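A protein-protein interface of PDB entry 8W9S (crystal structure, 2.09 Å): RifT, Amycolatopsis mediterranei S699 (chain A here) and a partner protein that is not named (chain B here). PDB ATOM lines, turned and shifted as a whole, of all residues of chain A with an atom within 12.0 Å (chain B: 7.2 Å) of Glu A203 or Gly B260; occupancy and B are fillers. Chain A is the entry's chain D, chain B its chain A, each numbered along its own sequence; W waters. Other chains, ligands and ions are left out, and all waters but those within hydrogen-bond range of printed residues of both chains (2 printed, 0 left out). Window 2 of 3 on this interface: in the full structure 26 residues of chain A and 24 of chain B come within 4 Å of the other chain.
Glu A203 touches just these residues of chain B: Gly B260 and Ser B261. No residue of chain A comes within 4 Å of Leu B152. No residue of chain A comes within 4 Å of Gly B257. No residue of chain A comes within 4 Å of Gly B259. Ser B261 touches just these residues of chain A: Gly A202 and Glu A203. Val B262 touches just one residue of chain A: Gly A201. Of the printed residues of chain B, Gly A202 touches Ser B261 (3.5 Å) and Ser B263 (3.97 Å). Printed residues of chain B within 4 Å of Leu A200: Ser B263 (3.2 Å). Of the printed residues of chain B, Gly A201 touches Val B262 (3.2 Å) and Ser B263 (2.8 Å).
N of Val B255 lies within hydrogen-bond range of O of Val B262 (2.9 Å). The side-chain hydroxyl (OG) of Ser B256 sits at hydrogen-bond distance from the side-chain hydroxyl (OG) of Ser B261, at 2.6 Å. The backbone carbonyl oxygen (O) of Leu A200 lies within hydrogen-bond range of the backbone NH (N) of Glu A206 (2.8 Å).
Among the printed residues, merely in contact across the chains: Leu A200 with Ser B263 (3.2 Å), Gly A201 with Val B262 (3.2 Å), Gly A202 with Ser B261 (3.5 Å), Gly A202 with Ser B263 (3.97 Å) and Glu A203 with Gly B260 (3.5 Å).
The backbone NH of Ser B261 lies within hydrogen-bond range of the side-chain carboxylate of Glu A203, at 2.7 Å. O of Ser B263 sits at hydrogen-bond distance from N of Gly A201 (2.8 Å).
Water W1 lies within hydrogen-bond range of the side-chain hydroxyl of Ser B261 (2.8 Å) and the side-chain carboxylate of Glu A203 (2.8 Å). Water W2 lies within hydrogen-bond range of the backbone NH (N) of Arg A204, the backbone carbonyl oxygen (O) of Ser B261 and the backbone NH (N) of Glu A203.
Of the 15 printed residues of chain B, 4 touch a printed residue of chain A. Hydrophobic or aromatic side chains of chain A within 4 Å of the printed part of chain B: Leu A200.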
ATOM      1  N   HIS A 173      29.873 -20.620 -11.760  1.00  0.00           N
ATOM      2  CA  HIS A 173      30.373 -19.504 -12.547  1.00  0.00           C
ATOM      3  C   HIS A 173      30.290 -18.260 -11.679  1.00  0.00           C
ATOM      4  O   HIS A 173      29.302 -18.063 -10.967  1.00  0.00           O
ATOM      5  CB  HIS A 173      29.579 -19.322 -13.849  1.00  0.00           C
ATOM      6  CG  HIS A 173      30.187 -18.338 -14.797  1.00  0.00           C
ATOM      7  ND1 HIS A 173      30.128 -16.974 -14.597  1.00  0.00           N
ATOM      8  CD2 HIS A 173      30.856 -18.518 -15.965  1.00  0.00           C
ATOM      9  CE1 HIS A 173      30.743 -16.357 -15.593  1.00  0.00           C
ATOM     10  NE2 HIS A 173      31.197 -17.271 -16.434  1.00  0.00           N
ATOM     11  N   SER A 175      29.657 -15.219 -12.192  1.00  0.00           N
ATOM     12  CA  SER A 175      28.580 -14.257 -12.382  1.00  0.00           C
ATOM     13  C   SER A 175      27.220 -14.931 -12.557  1.00  0.00           C
ATOM     14  O   SER A 175      26.259 -14.289 -12.986  1.00  0.00           O
ATOM     15  CB  SER A 175      28.918 -13.310 -13.540  1.00  0.00           C
ATOM     16  OG  SER A 175      29.123 -14.007 -14.741  1.00  0.00           O
ATOM     17  N   GLN A 198      16.172 -14.414 -20.464  1.00  0.00           N
ATOM     18  CA  GLN A 198      16.746 -13.200 -21.043  1.00  0.00           C
ATOM     19  C   GLN A 198      15.637 -12.220 -21.420  1.00  0.00           C
ATOM     20  O   GLN A 198      14.776 -12.524 -22.258  1.00  0.00           O
ATOM     21  CB  GLN A 198      17.593 -13.522 -22.274  1.00  0.00           C
ATOM     22  CG  GLN A 198      17.955 -12.264 -23.099  1.00  0.00           C
ATOM     23  CD  GLN A 198      18.789 -12.584 -24.344  1.00  0.00           C
ATOM     24  OE1 GLN A 198      19.927 -13.030 -24.229  1.00  0.00           O
ATOM     25  NE2 GLN A 198      18.227 -12.343 -25.530  1.00  0.00           N
ATOM     26  N   LEU A 199      15.670 -11.037 -20.811  1.00  0.00           N
ATOM     27  CA  LEU A 199      14.715  -9.985 -21.154  1.00  0.00           C
ATOM     28  C   LEU A 199      15.184  -9.197 -22.371  1.00  0.00           C
ATOM     29  O   LEU A 199      14.445  -9.050 -23.351  1.00  0.00           O
ATOM     30  CB  LEU A 199      14.528  -9.048 -19.960  1.00  0.00           C
ATOM     31  CG  LEU A 199      13.554  -7.868 -20.103  1.00  0.00           C
ATOM     32  CD1 LEU A 199      12.199  -8.354 -20.597  1.00  0.00           C
ATOM     33  CD2 LEU A 199      13.411  -7.104 -18.774  1.00  0.00           C
ATOM     34  N   LEU A 200      16.412  -8.683 -22.320  1.00  0.00           N
ATOM     35  CA  LEU A 200      17.011  -7.932 -23.417  1.00  0.00           C
ATOM     36  C   LEU A 200      18.299  -8.604 -23.889  1.00  0.00           C
ATOM     37  O   LEU A 200      19.116  -9.069 -23.080  1.00  0.00           O
ATOM     38  CB  LEU A 200      17.308  -6.475 -23.007  1.00  0.00           C
ATOM     39  CG  LEU A 200      16.132  -5.675 -22.433  1.00  0.00           C
ATOM     40  CD1 LEU A 200      16.568  -4.256 -22.019  1.00  0.00           C
ATOM     41  CD2 LEU A 200      14.980  -5.629 -23.415  1.00  0.00           C
ATOM     42  N   GLY A 201      18.466  -8.670 -25.204  1.00  0.00           N
ATOM     43  CA  GLY A 201      19.701  -9.118 -25.795  1.00  0.00           C
ATOM     44  C   GLY A 201      20.696  -7.991 -25.921  1.00  0.00           C
ATOM     45  O   GLY A 201      20.437  -6.836 -25.577  1.00  0.00           O
ATOM     46  N   GLY A 202      21.857  -8.338 -26.450  1.00  0.00           N
ATOM     47  CA  GLY A 202      22.918  -7.385 -26.668  1.00  0.00           C
ATOM     48  C   GLY A 202      24.224  -7.887 -26.099  1.00  0.00           C
ATOM     49  O   GLY A 202      24.350  -9.046 -25.691  1.00  0.00           O
ATOM     50  N   GLU A 203      25.220  -6.992 -26.075  1.00  0.00           N
ATOM     51  CA  GLU A 203      26.542  -7.366 -25.576  1.00  0.00           C
ATOM     52  C   GLU A 203      26.492  -7.710 -24.100  1.00  0.00           C
ATOM     53  O   GLU A 203      27.200  -8.615 -23.647  1.00  0.00           O
ATOM     54  CB  GLU A 203      27.552  -6.240 -25.832  1.00  0.00           C
ATOM     55  CG  GLU A 203      27.735  -5.901 -27.317  1.00  0.00           C
ATOM     56  CD  GLU A 203      27.120  -4.551 -27.684  1.00  0.00           C
ATOM     57  OE1 GLU A 203      27.823  -3.719 -28.307  1.00  0.00           O
ATOM     58  OE2 GLU A 203      25.939  -4.324 -27.324  1.00  0.00           O
ATOM     59  N   ARG A 204      25.652  -7.001 -23.334  1.00  0.00           N
ATOM     60  CA  ARG A 204      25.417  -7.245 -21.911  1.00  0.00           C
ATOM     61  C   ARG A 204      23.936  -7.580 -21.740  1.00  0.00           C
ATOM     62  O   ARG A 204      23.128  -6.692 -21.428  1.00  0.00           O
ATOM     63  CB  ARG A 204      25.786  -6.021 -21.073  1.00  0.00           C
ATOM     64  CG  ARG A 204      27.264  -5.853 -20.745  1.00  0.00           C
ATOM     65  CD  ARG A 204      27.449  -4.796 -19.657  1.00  0.00           C
ATOM     66  NE  ARG A 204      26.836  -5.215 -18.391  1.00  0.00           N
ATOM     67  CZ  ARG A 204      25.865  -4.557 -17.759  1.00  0.00           C
ATOM     68  NH1 ARG A 204      25.378  -5.039 -16.621  1.00  0.00           N
ATOM     69  NH2 ARG A 204      25.386  -3.418 -18.257  1.00  0.00           N
ATOM     70  N   PRO A 205      23.537  -8.840 -21.940  1.00  0.00           N
ATOM     71  CA  PRO A 205      22.106  -9.161 -21.902  1.00  0.00           C
ATOM     72  C   PRO A 205      21.515  -8.867 -20.534  1.00  0.00           C
ATOM     73  O   PRO A 205      22.213  -8.860 -19.521  1.00  0.00           O
ATOM     74  CB  PRO A 205      22.061 -10.657 -22.229  1.00  0.00           C
ATOM     75  CG  PRO A 205      23.367 -10.928 -22.926  1.00  0.00           C
ATOM     76  CD  PRO A 205      24.353 -10.021 -22.265  1.00  0.00           C
ATOM     77  N   GLU A 206      20.219  -8.586 -20.517  1.00  0.00           N
ATOM     78  CA  GLU A 206      19.523  -8.185 -19.306  1.00  0.00           C
ATOM     79  C   GLU A 206      18.601  -9.306 -18.873  1.00  0.00           C
ATOM     80  O   GLU A 206      17.900  -9.909 -19.694  1.00  0.00           O
ATOM     81  CB  GLU A 206      18.730  -6.897 -19.509  1.00  0.00           C
ATOM     82  CG  GLU A 206      19.596  -5.656 -19.466  1.00  0.00           C
ATOM     83  CD  GLU A 206      20.141  -5.384 -18.073  1.00  0.00           C
ATOM     84  OE1 GLU A 206      19.386  -5.578 -17.077  1.00  0.00           O
ATOM     85  OE2 GLU A 206      21.314  -4.956 -17.988  1.00  0.00           O
ATOM     86  N   LEU A 207      18.593  -9.567 -17.586  1.00  0.00           N
ATOM     87  CA  LEU A 207      17.939 -10.757 -17.090  1.00  0.00           C
ATOM     88  C   LEU A 207      16.498 -10.354 -16.800  1.00  0.00           C
ATOM     89  O   LEU A 207      16.256  -9.283 -16.247  1.00  0.00           O
ATOM     90  CB  LEU A 207      18.680 -11.232 -15.837  1.00  0.00           C
ATOM     91  CG  LEU A 207      18.547 -12.677 -15.439  1.00  0.00           C
ATOM     92  CD1 LEU A 207      19.327 -13.416 -16.558  1.00  0.00           C
ATOM     93  CD2 LEU A 207      19.122 -12.930 -14.070  1.00  0.00           C
ATOM     94  N   ARG B 151      24.314   3.690 -19.267  1.00  0.00           N
ATOM     95  CA  ARG B 151      24.829   2.382 -19.632  1.00  0.00           C
ATOM     96  C   ARG B 151      25.041   2.211 -21.129  1.00  0.00           C
ATOM     97  O   ARG B 151      25.908   1.427 -21.535  1.00  0.00           O
ATOM     98  CB  ARG B 151      23.884   1.262 -19.130  1.00  0.00           C
ATOM     99  CG  ARG B 151      23.860   1.140 -17.575  1.00  0.00           C
ATOM    100  CD  ARG B 151      25.191   0.504 -17.212  1.00  0.00           C
ATOM    101  NE  ARG B 151      25.239   0.105 -15.821  1.00  0.00           N
ATOM    102  CZ  ARG B 151      26.318  -0.344 -15.201  1.00  0.00           C
ATOM    103  NH1 ARG B 151      27.478  -0.241 -15.802  1.00  0.00           N
ATOM    104  NH2 ARG B 151      26.249  -0.727 -13.945  1.00  0.00           N
ATOM    105  N   LEU B 152      24.237   2.847 -21.973  1.00  0.00           N
ATOM    106  CA  LEU B 152      24.515   2.810 -23.405  1.00  0.00           C
ATOM    107  C   LEU B 152      25.328   3.988 -23.911  1.00  0.00           C
ATOM    108  O   LEU B 152      25.530   4.099 -25.129  1.00  0.00           O
ATOM    109  CB  LEU B 152      23.248   2.724 -24.253  1.00  0.00           C
ATOM    110  CG  LEU B 152      22.657   1.345 -24.545  1.00  0.00           C
ATOM    111  CD1 LEU B 152      21.869   0.705 -23.432  1.00  0.00           C
ATOM    112  CD2 LEU B 152      21.938   1.351 -25.898  1.00  0.00           C
ATOM    113  N   GLY B 153      25.808   4.861 -23.034  1.00  0.00           N
ATOM    114  CA  GLY B 153      26.512   6.010 -23.574  1.00  0.00           C
ATOM    115  C   GLY B 153      25.532   6.971 -24.228  1.00  0.00           C
ATOM    116  O   GLY B 153      24.391   7.124 -23.787  1.00  0.00           O
ATOM    117  N   GLU B 154      25.985   7.625 -25.301  1.00  0.00           N
ATOM    118  CA  GLU B 154      25.148   8.558 -26.053  1.00  0.00           C
ATOM    119  C   GLU B 154      24.310   7.790 -27.063  1.00  0.00           C
ATOM    120  O   GLU B 154      24.856   7.136 -27.958  1.00  0.00           O
ATOM    121  CB  GLU B 154      25.997   9.595 -26.792  1.00  0.00           C
ATOM    122  CG  GLU B 154      27.250  10.020 -26.069  1.00  0.00           C
ATOM    123  CD  GLU B 154      26.956  10.928 -24.899  1.00  0.00           C
ATOM    124  OE1 GLU B 154      25.832  11.480 -24.843  1.00  0.00           O
ATOM    125  OE2 GLU B 154      27.845  11.085 -24.028  1.00  0.00           O
ATOM    126  N   LEU B 157      20.953   5.438 -32.384  1.00  0.00           N
ATOM    127  CA  LEU B 157      20.111   4.836 -33.406  1.00  0.00           C
ATOM    128  C   LEU B 157      19.169   3.845 -32.753  1.00  0.00           C
ATOM    129  O   LEU B 157      19.603   3.002 -31.964  1.00  0.00           O
ATOM    130  CB  LEU B 157      20.959   4.126 -34.466  1.00  0.00           C
ATOM    131  CG  LEU B 157      20.133   3.308 -35.463  1.00  0.00           C
ATOM    132  CD1 LEU B 157      19.332   4.271 -36.330  1.00  0.00           C
ATOM    133  CD2 LEU B 157      21.010   2.389 -36.318  1.00  0.00           C
ATOM    134  N   HIS B 254      15.632  -2.459 -31.194  1.00  0.00           N
ATOM    135  CA  HIS B 254      17.084  -2.566 -31.171  1.00  0.00           C
ATOM    136  C   HIS B 254      17.624  -1.147 -31.074  1.00  0.00           C
ATOM    137  O   HIS B 254      17.333  -0.304 -31.932  1.00  0.00           O
ATOM    138  CB  HIS B 254      17.606  -3.292 -32.413  1.00  0.00           C
ATOM    139  CG  HIS B 254      19.091  -3.470 -32.423  1.00  0.00           C
ATOM    140  ND1 HIS B 254      19.700  -4.687 -32.180  1.00  0.00           N
ATOM    141  CD2 HIS B 254      20.091  -2.581 -32.622  1.00  0.00           C
ATOM    142  CE1 HIS B 254      21.012  -4.537 -32.239  1.00  0.00           C
ATOM    143  NE2 HIS B 254      21.273  -3.272 -32.518  1.00  0.00           N
ATOM    144  N   VAL B 255      18.360  -0.872 -30.003  1.00  0.00           N
ATOM    145  CA  VAL B 255      18.779   0.478 -29.663  1.00  0.00           C
ATOM    146  C   VAL B 255      20.291   0.483 -29.513  1.00  0.00           C
ATOM    147  O   VAL B 255      20.847  -0.378 -28.820  1.00  0.00           O
ATOM    148  CB  VAL B 255      18.091   0.950 -28.371  1.00  0.00           C
ATOM    149  CG1 VAL B 255      18.790   2.153 -27.785  1.00  0.00           C
ATOM    150  CG2 VAL B 255      16.620   1.260 -28.648  1.00  0.00           C
ATOM    151  N   SER B 256      20.954   1.449 -30.156  1.00  0.00           N
ATOM    152  CA  SER B 256      22.417   1.521 -30.153  1.00  0.00           C
ATOM    153  C   SER B 256      22.898   2.882 -29.669  1.00  0.00           C
ATOM    154  O   SER B 256      22.410   3.927 -30.119  1.00  0.00           O
ATOM    155  CB  SER B 256      23.012   1.263 -31.541  1.00  0.00           C
ATOM    156  OG  SER B 256      22.853  -0.081 -31.941  1.00  0.00           O
ATOM    157  N   GLY B 257      23.877   2.854 -28.764  1.00  0.00           N
ATOM    158  CA  GLY B 257      24.599   4.038 -28.360  1.00  0.00           C
ATOM    159  C   GLY B 257      26.094   3.760 -28.360  1.00  0.00           C
ATOM    160  O   GLY B 257      26.547   2.673 -28.739  1.00  0.00           O
ATOM    161  N   THR B 258      26.849   4.774 -27.919  1.00  0.00           N
ATOM    162  CA  THR B 258      28.303   4.652 -27.882  1.00  0.00           C
ATOM    163  C   THR B 258      28.761   3.552 -26.931  1.00  0.00           C
ATOM    164  O   THR B 258      29.851   3.011 -27.118  1.00  0.00           O
ATOM    165  CB  THR B 258      28.946   5.986 -27.480  1.00  0.00           C
ATOM    166  OG1 THR B 258      28.307   6.490 -26.301  1.00  0.00           O
ATOM    167  CG2 THR B 258      28.812   7.025 -28.621  1.00  0.00           C
ATOM    168  N   GLY B 259      27.953   3.205 -25.928  1.00  0.00           N
ATOM    169  CA  GLY B 259      28.266   2.179 -24.958  1.00  0.00           C
ATOM    170  C   GLY B 259      27.798   0.776 -25.297  1.00  0.00           C
ATOM    171  O   GLY B 259      28.017  -0.143 -24.500  1.00  0.00           O
ATOM    172  N   GLY B 260      27.160   0.578 -26.456  1.00  0.00           N
ATOM    173  CA  GLY B 260      26.747  -0.722 -26.931  1.00  0.00           C
ATOM    174  C   GLY B 260      25.306  -0.700 -27.420  1.00  0.00           C
ATOM    175  O   GLY B 260      24.754   0.361 -27.751  1.00  0.00           O
ATOM    176  N   SER B 261      24.707  -1.894 -27.455  1.00  0.00           N
ATOM    177  CA  SER B 261      23.389  -2.129 -28.028  1.00  0.00           C
ATOM    178  C   SER B 261      22.585  -3.052 -27.130  1.00  0.00           C
ATOM    179  O   SER B 261      23.142  -3.924 -26.458  1.00  0.00           O
ATOM    180  CB  SER B 261      23.471  -2.783 -29.408  1.00  0.00           C
ATOM    181  OG  SER B 261      23.966  -1.876 -30.359  1.00  0.00           O
ATOM    182  N   VAL B 262      21.265  -2.860 -27.141  1.00  0.00           N
ATOM    183  CA  VAL B 262      20.331  -3.773 -26.494  1.00  0.00           C
ATOM    184  C   VAL B 262      19.142  -3.972 -27.419  1.00  0.00           C
ATOM    185  O   VAL B 262      18.740  -3.066 -28.159  1.00  0.00           O
ATOM    186  CB  VAL B 262      19.866  -3.276 -25.103  1.00  0.00           C
ATOM    187  CG1 VAL B 262      21.003  -3.436 -24.078  1.00  0.00           C
ATOM    188  CG2 VAL B 262      19.420  -1.830 -25.186  1.00  0.00           C
ATOM    189  N   SER B 263      18.583  -5.175 -27.372  1.00  0.00           N
ATOM    190  CA  SER B 263      17.535  -5.595 -28.278  1.00  0.00           C
ATOM    191  C   SER B 263      16.456  -6.336 -27.503  1.00  0.00           C
ATOM    192  O   SER B 263      16.666  -6.795 -26.370  1.00  0.00           O
ATOM    193  CB  SER B 263      18.091  -6.504 -29.373  1.00  0.00           C
ATOM    194  OG  SER B 263      18.714  -7.612 -28.756  1.00  0.00           O
HETATM  195  O   HOH W   1      26.785  -1.791 -30.126  1.00  0.00           O
HETATM  196  O   HOH W   2      24.574  -4.409 -23.970  1.00  0.00           O
